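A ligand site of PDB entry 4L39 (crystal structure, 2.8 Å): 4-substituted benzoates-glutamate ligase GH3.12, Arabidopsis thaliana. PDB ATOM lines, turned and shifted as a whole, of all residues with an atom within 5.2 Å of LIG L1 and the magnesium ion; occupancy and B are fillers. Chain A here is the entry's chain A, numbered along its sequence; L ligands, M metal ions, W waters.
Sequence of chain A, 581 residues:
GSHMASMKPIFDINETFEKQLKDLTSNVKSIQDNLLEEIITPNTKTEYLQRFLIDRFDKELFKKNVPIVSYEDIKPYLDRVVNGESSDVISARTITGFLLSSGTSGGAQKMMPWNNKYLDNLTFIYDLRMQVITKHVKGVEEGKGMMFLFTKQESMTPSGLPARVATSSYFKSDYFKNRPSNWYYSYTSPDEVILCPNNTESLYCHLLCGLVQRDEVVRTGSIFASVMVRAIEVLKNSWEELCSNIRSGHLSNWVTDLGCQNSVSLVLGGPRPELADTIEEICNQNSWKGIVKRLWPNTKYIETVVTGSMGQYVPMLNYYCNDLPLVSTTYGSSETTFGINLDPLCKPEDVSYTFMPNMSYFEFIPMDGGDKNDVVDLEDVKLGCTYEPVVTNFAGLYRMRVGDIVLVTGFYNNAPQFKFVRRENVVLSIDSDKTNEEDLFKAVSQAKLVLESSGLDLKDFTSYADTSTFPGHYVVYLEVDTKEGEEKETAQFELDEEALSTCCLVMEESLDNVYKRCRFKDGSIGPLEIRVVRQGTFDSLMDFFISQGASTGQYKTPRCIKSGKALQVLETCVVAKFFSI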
ATOM      1  N   LEU A 100      37.984 -22.131 -13.958  1.00  0.00           N
ATOM      2  CA  LEU A 100      38.453 -20.798 -14.254  1.00  0.00           C
ATOM      3  C   LEU A 100      37.357 -19.796 -14.033  1.00  0.00           C
ATOM      4  O   LEU A 100      36.228 -20.010 -14.456  1.00  0.00           O
ATOM      5  CB  LEU A 100      38.891 -20.710 -15.711  1.00  0.00           C
ATOM      6  CG  LEU A 100      40.159 -21.439 -16.152  1.00  0.00           C
ATOM      7  CD1 LEU A 100      40.145 -21.515 -17.641  1.00  0.00           C
ATOM      8  CD2 LEU A 100      41.317 -20.707 -15.715  1.00  0.00           C
ATOM      9  N   SER A 101      37.710 -18.673 -13.397  1.00  0.00           N
ATOM     10  CA  SER A 101      36.832 -17.513 -13.310  1.00  0.00           C
ATOM     11  C   SER A 101      36.720 -16.811 -14.665  1.00  0.00           C
ATOM     12  O   SER A 101      36.409 -15.616 -14.718  1.00  0.00           O
ATOM     13  CB  SER A 101      37.356 -16.521 -12.267  1.00  0.00           C
ATOM     14  OG  SER A 101      37.497 -17.121 -10.994  1.00  0.00           O
ATOM     15  N   MET A 112      39.956 -22.139  -9.038  1.00  0.00           N
ATOM     16  CA  MET A 112      39.312 -22.764  -7.905  1.00  0.00           C
ATOM     17  C   MET A 112      39.414 -24.272  -8.087  1.00  0.00           C
ATOM     18  O   MET A 112      39.308 -24.771  -9.212  1.00  0.00           O
ATOM     19  CB  MET A 112      37.840 -22.364  -7.893  1.00  0.00           C
ATOM     20  CG  MET A 112      37.609 -20.887  -7.806  1.00  0.00           C
ATOM     21  SD  MET A 112      38.005 -20.316  -6.167  1.00  0.00           S
ATOM     22  CE  MET A 112      38.158 -18.561  -6.474  1.00  0.00           C
ATOM     23  N   ALA A 166      33.101 -23.029 -15.646  1.00  0.00           N
ATOM     24  CA  ALA A 166      32.024 -23.813 -14.976  1.00  0.00           C
ATOM     25  C   ALA A 166      31.185 -24.723 -15.905  1.00  0.00           C
ATOM     26  O   ALA A 166      31.050 -25.911 -15.643  1.00  0.00           O
ATOM     27  CB  ALA A 166      31.105 -22.869 -14.165  1.00  0.00           C
ATOM     28  N   PHE A 224      24.214 -16.364 -19.730  1.00  0.00           N
ATOM     29  CA  PHE A 224      24.064 -14.920 -19.483  1.00  0.00           C
ATOM     30  C   PHE A 224      23.465 -14.179 -20.694  1.00  0.00           C
ATOM     31  O   PHE A 224      23.544 -14.665 -21.831  1.00  0.00           O
ATOM     32  CB  PHE A 224      25.397 -14.290 -19.053  1.00  0.00           C
ATOM     33  CG  PHE A 224      25.900 -14.789 -17.713  1.00  0.00           C
ATOM     34  CD1 PHE A 224      25.323 -14.338 -16.536  1.00  0.00           C
ATOM     35  CD2 PHE A 224      26.964 -15.699 -17.645  1.00  0.00           C
ATOM     36  CE1 PHE A 224      25.777 -14.801 -15.330  1.00  0.00           C
ATOM     37  CE2 PHE A 224      27.417 -16.174 -16.434  1.00  0.00           C
ATOM     38  CZ  PHE A 224      26.827 -15.730 -15.270  1.00  0.00           C
ATOM     39  N   VAL A 305      20.061 -15.202 -17.750  1.00  0.00           N
ATOM     40  CA  VAL A 305      20.170 -14.388 -16.559  1.00  0.00           C
ATOM     41  C   VAL A 305      20.185 -12.912 -16.950  1.00  0.00           C
ATOM     42  O   VAL A 305      20.949 -12.525 -17.814  1.00  0.00           O
ATOM     43  CB  VAL A 305      21.461 -14.794 -15.766  1.00  0.00           C
ATOM     44  CG1 VAL A 305      21.915 -13.711 -14.759  1.00  0.00           C
ATOM     45  CG2 VAL A 305      21.234 -16.076 -15.016  1.00  0.00           C
ATOM     46  N   THR A 307      19.835 -10.542 -14.120  1.00  0.00           N
ATOM     47  CA  THR A 307      20.052  -9.887 -12.840  1.00  0.00           C
ATOM     48  C   THR A 307      21.485  -9.357 -12.764  1.00  0.00           C
ATOM     49  O   THR A 307      22.254  -9.595 -13.668  1.00  0.00           O
ATOM     50  CB  THR A 307      19.664 -10.811 -11.652  1.00  0.00           C
ATOM     51  OG1 THR A 307      20.435 -12.017 -11.652  1.00  0.00           O
ATOM     52  CG2 THR A 307      18.242 -11.169 -11.795  1.00  0.00           C
ATOM     53  N   GLY A 308      21.825  -8.615 -11.712  1.00  0.00           N
ATOM     54  CA  GLY A 308      23.083  -7.895 -11.659  1.00  0.00           C
ATOM     55  C   GLY A 308      23.341  -7.035 -12.894  1.00  0.00           C
ATOM     56  O   GLY A 308      22.419  -6.492 -13.512  1.00  0.00           O
ATOM     57  N   THR A 330      19.110 -19.161 -12.086  1.00  0.00           N
ATOM     58  CA  THR A 330      20.124 -19.700 -11.186  1.00  0.00           C
ATOM     59  C   THR A 330      21.113 -18.668 -10.757  1.00  0.00           C
ATOM     60  O   THR A 330      21.457 -17.764 -11.514  1.00  0.00           O
ATOM     61  CB  THR A 330      20.961 -20.794 -11.899  1.00  0.00           C
ATOM     62  OG1 THR A 330      20.095 -21.817 -12.426  1.00  0.00           O
ATOM     63  CG2 THR A 330      21.948 -21.405 -10.951  1.00  0.00           C
ATOM     64  N   TYR A 331      21.592 -18.817  -9.539  1.00  0.00           N
ATOM     65  CA  TYR A 331      22.693 -17.995  -9.074  1.00  0.00           C
ATOM     66  C   TYR A 331      23.879 -18.914  -8.657  1.00  0.00           C
ATOM     67  O   TYR A 331      23.730 -19.856  -7.855  1.00  0.00           O
ATOM     68  CB  TYR A 331      22.186 -17.046  -7.975  1.00  0.00           C
ATOM     69  CG  TYR A 331      23.282 -16.266  -7.242  1.00  0.00           C
ATOM     70  CD1 TYR A 331      24.474 -15.892  -7.871  1.00  0.00           C
ATOM     71  CD2 TYR A 331      23.126 -15.942  -5.901  1.00  0.00           C
ATOM     72  CE1 TYR A 331      25.473 -15.215  -7.184  1.00  0.00           C
ATOM     73  CE2 TYR A 331      24.108 -15.264  -5.212  1.00  0.00           C
ATOM     74  CZ  TYR A 331      25.275 -14.904  -5.854  1.00  0.00           C
ATOM     75  OH  TYR A 331      26.230 -14.235  -5.134  1.00  0.00           O
ATOM     76  N   GLY A 332      25.036 -18.651  -9.255  1.00  0.00           N
ATOM     77  CA  GLY A 332      26.179 -19.533  -9.115  1.00  0.00           C
ATOM     78  C   GLY A 332      27.562 -18.978  -9.424  1.00  0.00           C
ATOM     79  O   GLY A 332      27.728 -17.924 -10.027  1.00  0.00           O
ATOM     80  N   SER A 333      28.574 -19.703  -8.973  1.00  0.00           N
ATOM     81  CA  SER A 333      29.934 -19.267  -9.138  1.00  0.00           C
ATOM     82  C   SER A 333      30.800 -20.492  -9.164  1.00  0.00           C
ATOM     83  O   SER A 333      30.306 -21.645  -9.144  1.00  0.00           O
ATOM     84  CB  SER A 333      30.356 -18.469  -7.955  1.00  0.00           C
ATOM     85  OG  SER A 333      30.394 -19.315  -6.831  1.00  0.00           O
ATOM     86  N   SER A 334      32.093 -20.214  -9.197  1.00  0.00           N
ATOM     87  CA  SER A 334      33.107 -21.251  -9.212  1.00  0.00           C
ATOM     88  C   SER A 334      33.280 -21.835  -7.827  1.00  0.00           C
ATOM     89  O   SER A 334      33.656 -22.965  -7.691  1.00  0.00           O
ATOM     90  CB  SER A 334      34.453 -20.694  -9.695  1.00  0.00           C
ATOM     91  OG  SER A 334      34.357 -20.144 -11.006  1.00  0.00           O
ATOM     92  N   GLU A 335      32.998 -21.057  -6.780  1.00  0.00           N
ATOM     93  CA  GLU A 335      32.955 -21.584  -5.416  1.00  0.00           C
ATOM     94  C   GLU A 335      31.790 -22.547  -5.291  1.00  0.00           C
ATOM     95  O   GLU A 335      31.922 -23.621  -4.723  1.00  0.00           O
ATOM     96  CB  GLU A 335      32.769 -20.497  -4.364  1.00  0.00           C
ATOM     97  CG  GLU A 335      33.802 -19.383  -4.384  1.00  0.00           C
ATOM     98  CD  GLU A 335      33.426 -18.272  -5.357  1.00  0.00           C
ATOM     99  OE1 GLU A 335      32.371 -17.624  -5.153  1.00  0.00           O
ATOM    100  OE2 GLU A 335      34.174 -18.057  -6.347  1.00  0.00           O
ATOM    101  N   TYR A 353      16.824 -15.270  -5.404  1.00  0.00           N
ATOM    102  CA  TYR A 353      17.343 -16.627  -5.465  1.00  0.00           C
ATOM    103  C   TYR A 353      17.221 -17.253  -4.092  1.00  0.00           C
ATOM    104  O   TYR A 353      17.701 -16.684  -3.127  1.00  0.00           O
ATOM    105  CB  TYR A 353      18.788 -16.642  -5.931  1.00  0.00           C
ATOM    106  CG  TYR A 353      18.947 -16.007  -7.286  1.00  0.00           C
ATOM    107  CD1 TYR A 353      18.616 -16.719  -8.422  1.00  0.00           C
ATOM    108  CD2 TYR A 353      19.413 -14.696  -7.447  1.00  0.00           C
ATOM    109  CE1 TYR A 353      18.741 -16.166  -9.686  1.00  0.00           C
ATOM    110  CE2 TYR A 353      19.557 -14.132  -8.706  1.00  0.00           C
ATOM    111  CZ  TYR A 353      19.214 -14.877  -9.829  1.00  0.00           C
ATOM    112  OH  TYR A 353      19.317 -14.396 -11.110  1.00  0.00           O
ATOM    113  N   MET A 400      35.355 -19.066   2.521  1.00  0.00           N
ATOM    114  CA  MET A 400      35.840 -18.228   1.444  1.00  0.00           C
ATOM    115  C   MET A 400      34.793 -17.155   1.065  1.00  0.00           C
ATOM    116  O   MET A 400      33.666 -17.478   0.741  1.00  0.00           O
ATOM    117  CB  MET A 400      36.142 -19.179   0.282  1.00  0.00           C
ATOM    118  CG  MET A 400      36.234 -18.560  -1.088  1.00  0.00           C
ATOM    119  SD  MET A 400      37.728 -17.634  -1.332  1.00  0.00           S
ATOM    120  CE  MET A 400      37.526 -17.315  -3.069  1.00  0.00           C
ATOM    121  N   ARG A 401      35.168 -15.870   1.176  1.00  0.00           N
ATOM    122  CA  ARG A 401      34.343 -14.729   0.734  1.00  0.00           C
ATOM    123  C   ARG A 401      34.061 -14.682  -0.800  1.00  0.00           C
ATOM    124  O   ARG A 401      34.970 -14.754  -1.658  1.00  0.00           O
ATOM    125  CB  ARG A 401      35.023 -13.428   1.161  1.00  0.00           C
ATOM    126  CG  ARG A 401      34.729 -13.067   2.549  1.00  0.00           C
ATOM    127  CD  ARG A 401      35.791 -12.137   3.090  1.00  0.00           C
ATOM    128  NE  ARG A 401      35.930 -10.947   2.265  1.00  0.00           N
ATOM    129  CZ  ARG A 401      35.581  -9.731   2.631  1.00  0.00           C
ATOM    130  NH1 ARG A 401      35.040  -9.513   3.844  1.00  0.00           N
ATOM    131  NH2 ARG A 401      35.774  -8.731   1.785  1.00  0.00           N
ATOM    132  N   VAL A 402      32.793 -14.517  -1.150  1.00  0.00           N
ATOM    133  CA  VAL A 402      32.399 -14.698  -2.517  1.00  0.00           C
ATOM    134  C   VAL A 402      32.535 -13.404  -3.256  1.00  0.00           C
ATOM    135  O   VAL A 402      32.796 -13.420  -4.451  1.00  0.00           O
ATOM    136  CB  VAL A 402      30.970 -15.223  -2.615  1.00  0.00           C
ATOM    137  CG1 VAL A 402      30.517 -15.258  -4.086  1.00  0.00           C
ATOM    138  CG2 VAL A 402      30.881 -16.622  -1.932  1.00  0.00           C
ATOM    139  N   GLY A 403      32.374 -12.285  -2.548  1.00  0.00           N
ATOM    140  CA  GLY A 403      32.436 -10.971  -3.177  1.00  0.00           C
ATOM    141  C   GLY A 403      31.200 -10.625  -3.967  1.00  0.00           C
ATOM    142  O   GLY A 403      31.265 -10.040  -5.065  1.00  0.00           O
ATOM    143  N   ASP A 404      30.055 -11.003  -3.429  1.00  0.00           N
ATOM    144  CA  ASP A 404      28.793 -10.469  -3.909  1.00  0.00           C
ATOM    145  C   ASP A 404      28.121  -9.918  -2.685  1.00  0.00           C
ATOM    146  O   ASP A 404      28.406 -10.365  -1.588  1.00  0.00           O
ATOM    147  CB  ASP A 404      27.950 -11.566  -4.559  1.00  0.00           C
ATOM    148  CG  ASP A 404      28.529 -12.058  -5.854  1.00  0.00           C
ATOM    149  OD1 ASP A 404      29.024 -11.203  -6.602  1.00  0.00           O
ATOM    150  OD2 ASP A 404      28.522 -13.276  -6.130  1.00  0.00           O
ATOM    151  N   PHE A 420      20.090 -10.414  -5.619  1.00  0.00           N
ATOM    152  CA  PHE A 420      21.449 -10.104  -5.993  1.00  0.00           C
ATOM    153  C   PHE A 420      21.562  -8.590  -6.214  1.00  0.00           C
ATOM    154  O   PHE A 420      20.844  -8.031  -7.032  1.00  0.00           O
ATOM    155  CB  PHE A 420      21.862 -10.829  -7.229  1.00  0.00           C
ATOM    156  CG  PHE A 420      23.292 -10.610  -7.568  1.00  0.00           C
ATOM    157  CD1 PHE A 420      24.274 -11.540  -7.150  1.00  0.00           C
ATOM    158  CD2 PHE A 420      23.677  -9.450  -8.267  1.00  0.00           C
ATOM    159  CE1 PHE A 420      25.594 -11.346  -7.472  1.00  0.00           C
ATOM    160  CE2 PHE A 420      24.978  -9.223  -8.570  1.00  0.00           C
ATOM    161  CZ  PHE A 420      25.960 -10.171  -8.189  1.00  0.00           C
ATOM    162  N   ARG A 423      28.318  -6.763  -7.196  1.00  0.00           N
ATOM    163  CA  ARG A 423      29.581  -7.458  -6.999  1.00  0.00           C
ATOM    164  C   ARG A 423      30.513  -6.526  -6.222  1.00  0.00           C
ATOM    165  O   ARG A 423      30.836  -5.458  -6.721  1.00  0.00           O
ATOM    166  CB  ARG A 423      30.154  -7.816  -8.340  1.00  0.00           C
ATOM    167  N   SER A 432      31.770 -11.709 -20.248  1.00  0.00           N
ATOM    168  CA  SER A 432      32.440 -12.583 -19.284  1.00  0.00           C
ATOM    169  C   SER A 432      33.462 -11.795 -18.435  1.00  0.00           C
ATOM    170  O   SER A 432      33.654 -12.064 -17.242  1.00  0.00           O
ATOM    171  CB  SER A 432      33.139 -13.727 -20.013  1.00  0.00           C
ATOM    172  N   LYS A 434      35.611  -9.525 -16.133  1.00  0.00           N
ATOM    173  CA  LYS A 434      35.451  -8.810 -14.876  1.00  0.00           C
ATOM    174  C   LYS A 434      36.657  -7.891 -14.688  1.00  0.00           C
ATOM    175  O   LYS A 434      37.769  -8.363 -14.465  1.00  0.00           O
ATOM    176  CB  LYS A 434      35.328  -9.779 -13.693  1.00  0.00           C
HETATM  177  P1  LIG L   1      35.529 -13.467  -9.518  1.00  0.00           P
HETATM  178  O1  LIG L   1      35.079 -12.017  -9.708  1.00  0.00           O
HETATM  179  O2  LIG L   1      35.364 -13.846  -8.058  1.00  0.00           O
HETATM  180  O3  LIG L   1      36.981 -13.528  -9.966  1.00  0.00           O
HETATM  181  P2  LIG L   1      34.015 -14.237 -11.794  1.00  0.00           P
HETATM  182  O4  LIG L   1      32.801 -13.376 -11.534  1.00  0.00           O
HETATM  183  O5  LIG L   1      34.973 -13.448 -12.693  1.00  0.00           O
HETATM  184  O6  LIG L   1      34.669 -14.519 -10.384  1.00  0.00           O
HETATM  185  P3  LIG L   1      32.548 -16.882 -11.611  1.00  0.00           P
HETATM  186  O7  LIG L   1      32.250 -18.154 -12.365  1.00  0.00           O
HETATM  187  O8  LIG L   1      33.249 -17.113 -10.260  1.00  0.00           O
HETATM  188  C1  LIG L   1      33.606 -15.797 -12.700  1.00  0.00           C
HETATM  189  O9  LIG L   1      31.150 -16.145 -11.540  1.00  0.00           O
HETATM  190  C2  LIG L   1      30.416 -15.893 -10.345  1.00  0.00           C
HETATM  191  C3  LIG L   1      29.910 -14.525 -10.378  1.00  0.00           C
HETATM  192  O10 LIG L   1      29.054 -14.235 -11.586  1.00  0.00           O
HETATM  193  C4  LIG L   1      29.078 -14.407  -9.182  1.00  0.00           C
HETATM  194  O11 LIG L   1      29.914 -13.874  -8.139  1.00  0.00           O
HETATM  195  C5  LIG L   1      28.049 -13.478  -9.552  1.00  0.00           C
HETATM  196  O12 LIG L   1      28.631 -12.229  -9.197  1.00  0.00           O
HETATM  197  C6  LIG L   1      27.840 -13.539 -11.017  1.00  0.00           C
HETATM  198  N1  LIG L   1      26.661 -14.230 -11.256  1.00  0.00           N
HETATM  199  C7  LIG L   1      26.501 -15.528 -11.564  1.00  0.00           C
HETATM  200  N2  LIG L   1      25.223 -15.808 -11.696  1.00  0.00           N
HETATM  201  C8  LIG L   1      24.520 -14.723 -11.478  1.00  0.00           C
HETATM  202  C9  LIG L   1      23.171 -14.409 -11.486  1.00  0.00           C
HETATM  203  N3  LIG L   1      22.234 -15.399 -11.732  1.00  0.00           N
HETATM  204  N4  LIG L   1      22.740 -13.168 -11.230  1.00  0.00           N
HETATM  205  C10 LIG L   1      23.587 -12.143 -10.971  1.00  0.00           C
HETATM  206  N5  LIG L   1      24.918 -12.399 -10.942  1.00  0.00           N
HETATM  207  C11 LIG L   1      25.400 -13.668 -11.192  1.00  0.00           C
HETATM  208  C1  LG2 L   2      24.324 -22.856 -15.241  1.00  0.00           C
HETATM  209  O1  LG2 L   2      24.944 -23.962 -15.273  1.00  0.00           O
HETATM  210  O2  LG2 L   2      23.320 -22.706 -15.972  1.00  0.00           O
HETATM  211  C2  LG2 L   2      24.876 -21.740 -14.349  1.00  0.00           C
HETATM  212  C3  LG2 L   2      24.210 -20.540 -14.105  1.00  0.00           C
HETATM  213  C4  LG2 L   2      24.730 -19.528 -13.296  1.00  0.00           C
HETATM  214  C5  LG2 L   2      25.972 -19.708 -12.716  1.00  0.00           C
HETATM  215  C6  LG2 L   2      26.658 -20.885 -12.947  1.00  0.00           C
HETATM  216  C7  LG2 L   2      26.120 -21.897 -13.753  1.00  0.00           C
HETATM  217  O3  LG2 L   2      22.956 -20.355 -14.691  1.00  0.00           O
HETATM  218 MG    MG M   1      35.102 -14.553  -5.776  1.00  0.00          MG
HETATM  219  O   HOH W   1      32.288 -12.200  -7.384  1.00  0.00           O
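The magnesium ion is bound by O2 of LIG L1 (2.4 Å).
O of Thr 330 is in hydrogen-bond range of N3 of LIG L1. OD2 of Asp 404 is in hydrogen-bond range of O11 of LIG L1. OG1 of Thr 307 sits at hydrogen-bond distance from N4 of LIG L1 (2.6 Å). The side-chain hydroxyl (OH) of Tyr 353 lies within hydrogen-bond range of a nitrogen (N3) of LIG L1, 3.1 Å away. An oxygen (O8) of LIG L1 is in hydrogen-bond range of the backbone NH (N) of Ser 334, at 3.5 Å. OG of Ser 334 is in hydrogen-bond range of O7 of LIG L1 (3.2 Å).
OE2 of Glu 335 touches the magnesium ion, 3.7 Å away. Val 402 touches the magnesium ion (O to MG, 2.9 Å). Of the 24 residues printed, 2 come within 4 Å of the magnesium ion. The nearest printed residue that does not touch the magnesium ion is Arg 401 (4.1 Å).
Water W1 lies within hydrogen-bond range of O11 of LIG L1, O of Val 402 and O of Gly 403.
O of Ser 101 sits close to O5 of LIG L1 (3.3 Å). CZ of Phe 224 touches C7 of LIG L1, 3.7 Å away. Val 305 touches LIG L1. CA of Tyr 331 touches N3 of LIG L1, 3.7 Å away. Gly 332 touches LIG L1 (O to C7, 3.1 Å). Ser 333 touches LIG L1 (CB to C2, 3.5 Å). Phe 420 touches LIG L1 (CZ to O12, 3.5 Å). Lys 434 touches LIG L1. The nearest printed residue that does not touch LIG L1 is Gly 308 (4.01 Å).
OH of Tyr 331 lies within hydrogen-bond range of OD2 of Asp 404. The side-chain hydroxyl (OH) of Tyr 353 is in hydrogen-bond range of the side-chain hydroxyl (OG1) of Thr 307 (2.7 Å). The side-chain carboxylate (OE1) of Glu 335 sits at hydrogen-bond distance from the side-chain hydroxyl (OG) of Ser 333 (3.1 Å).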
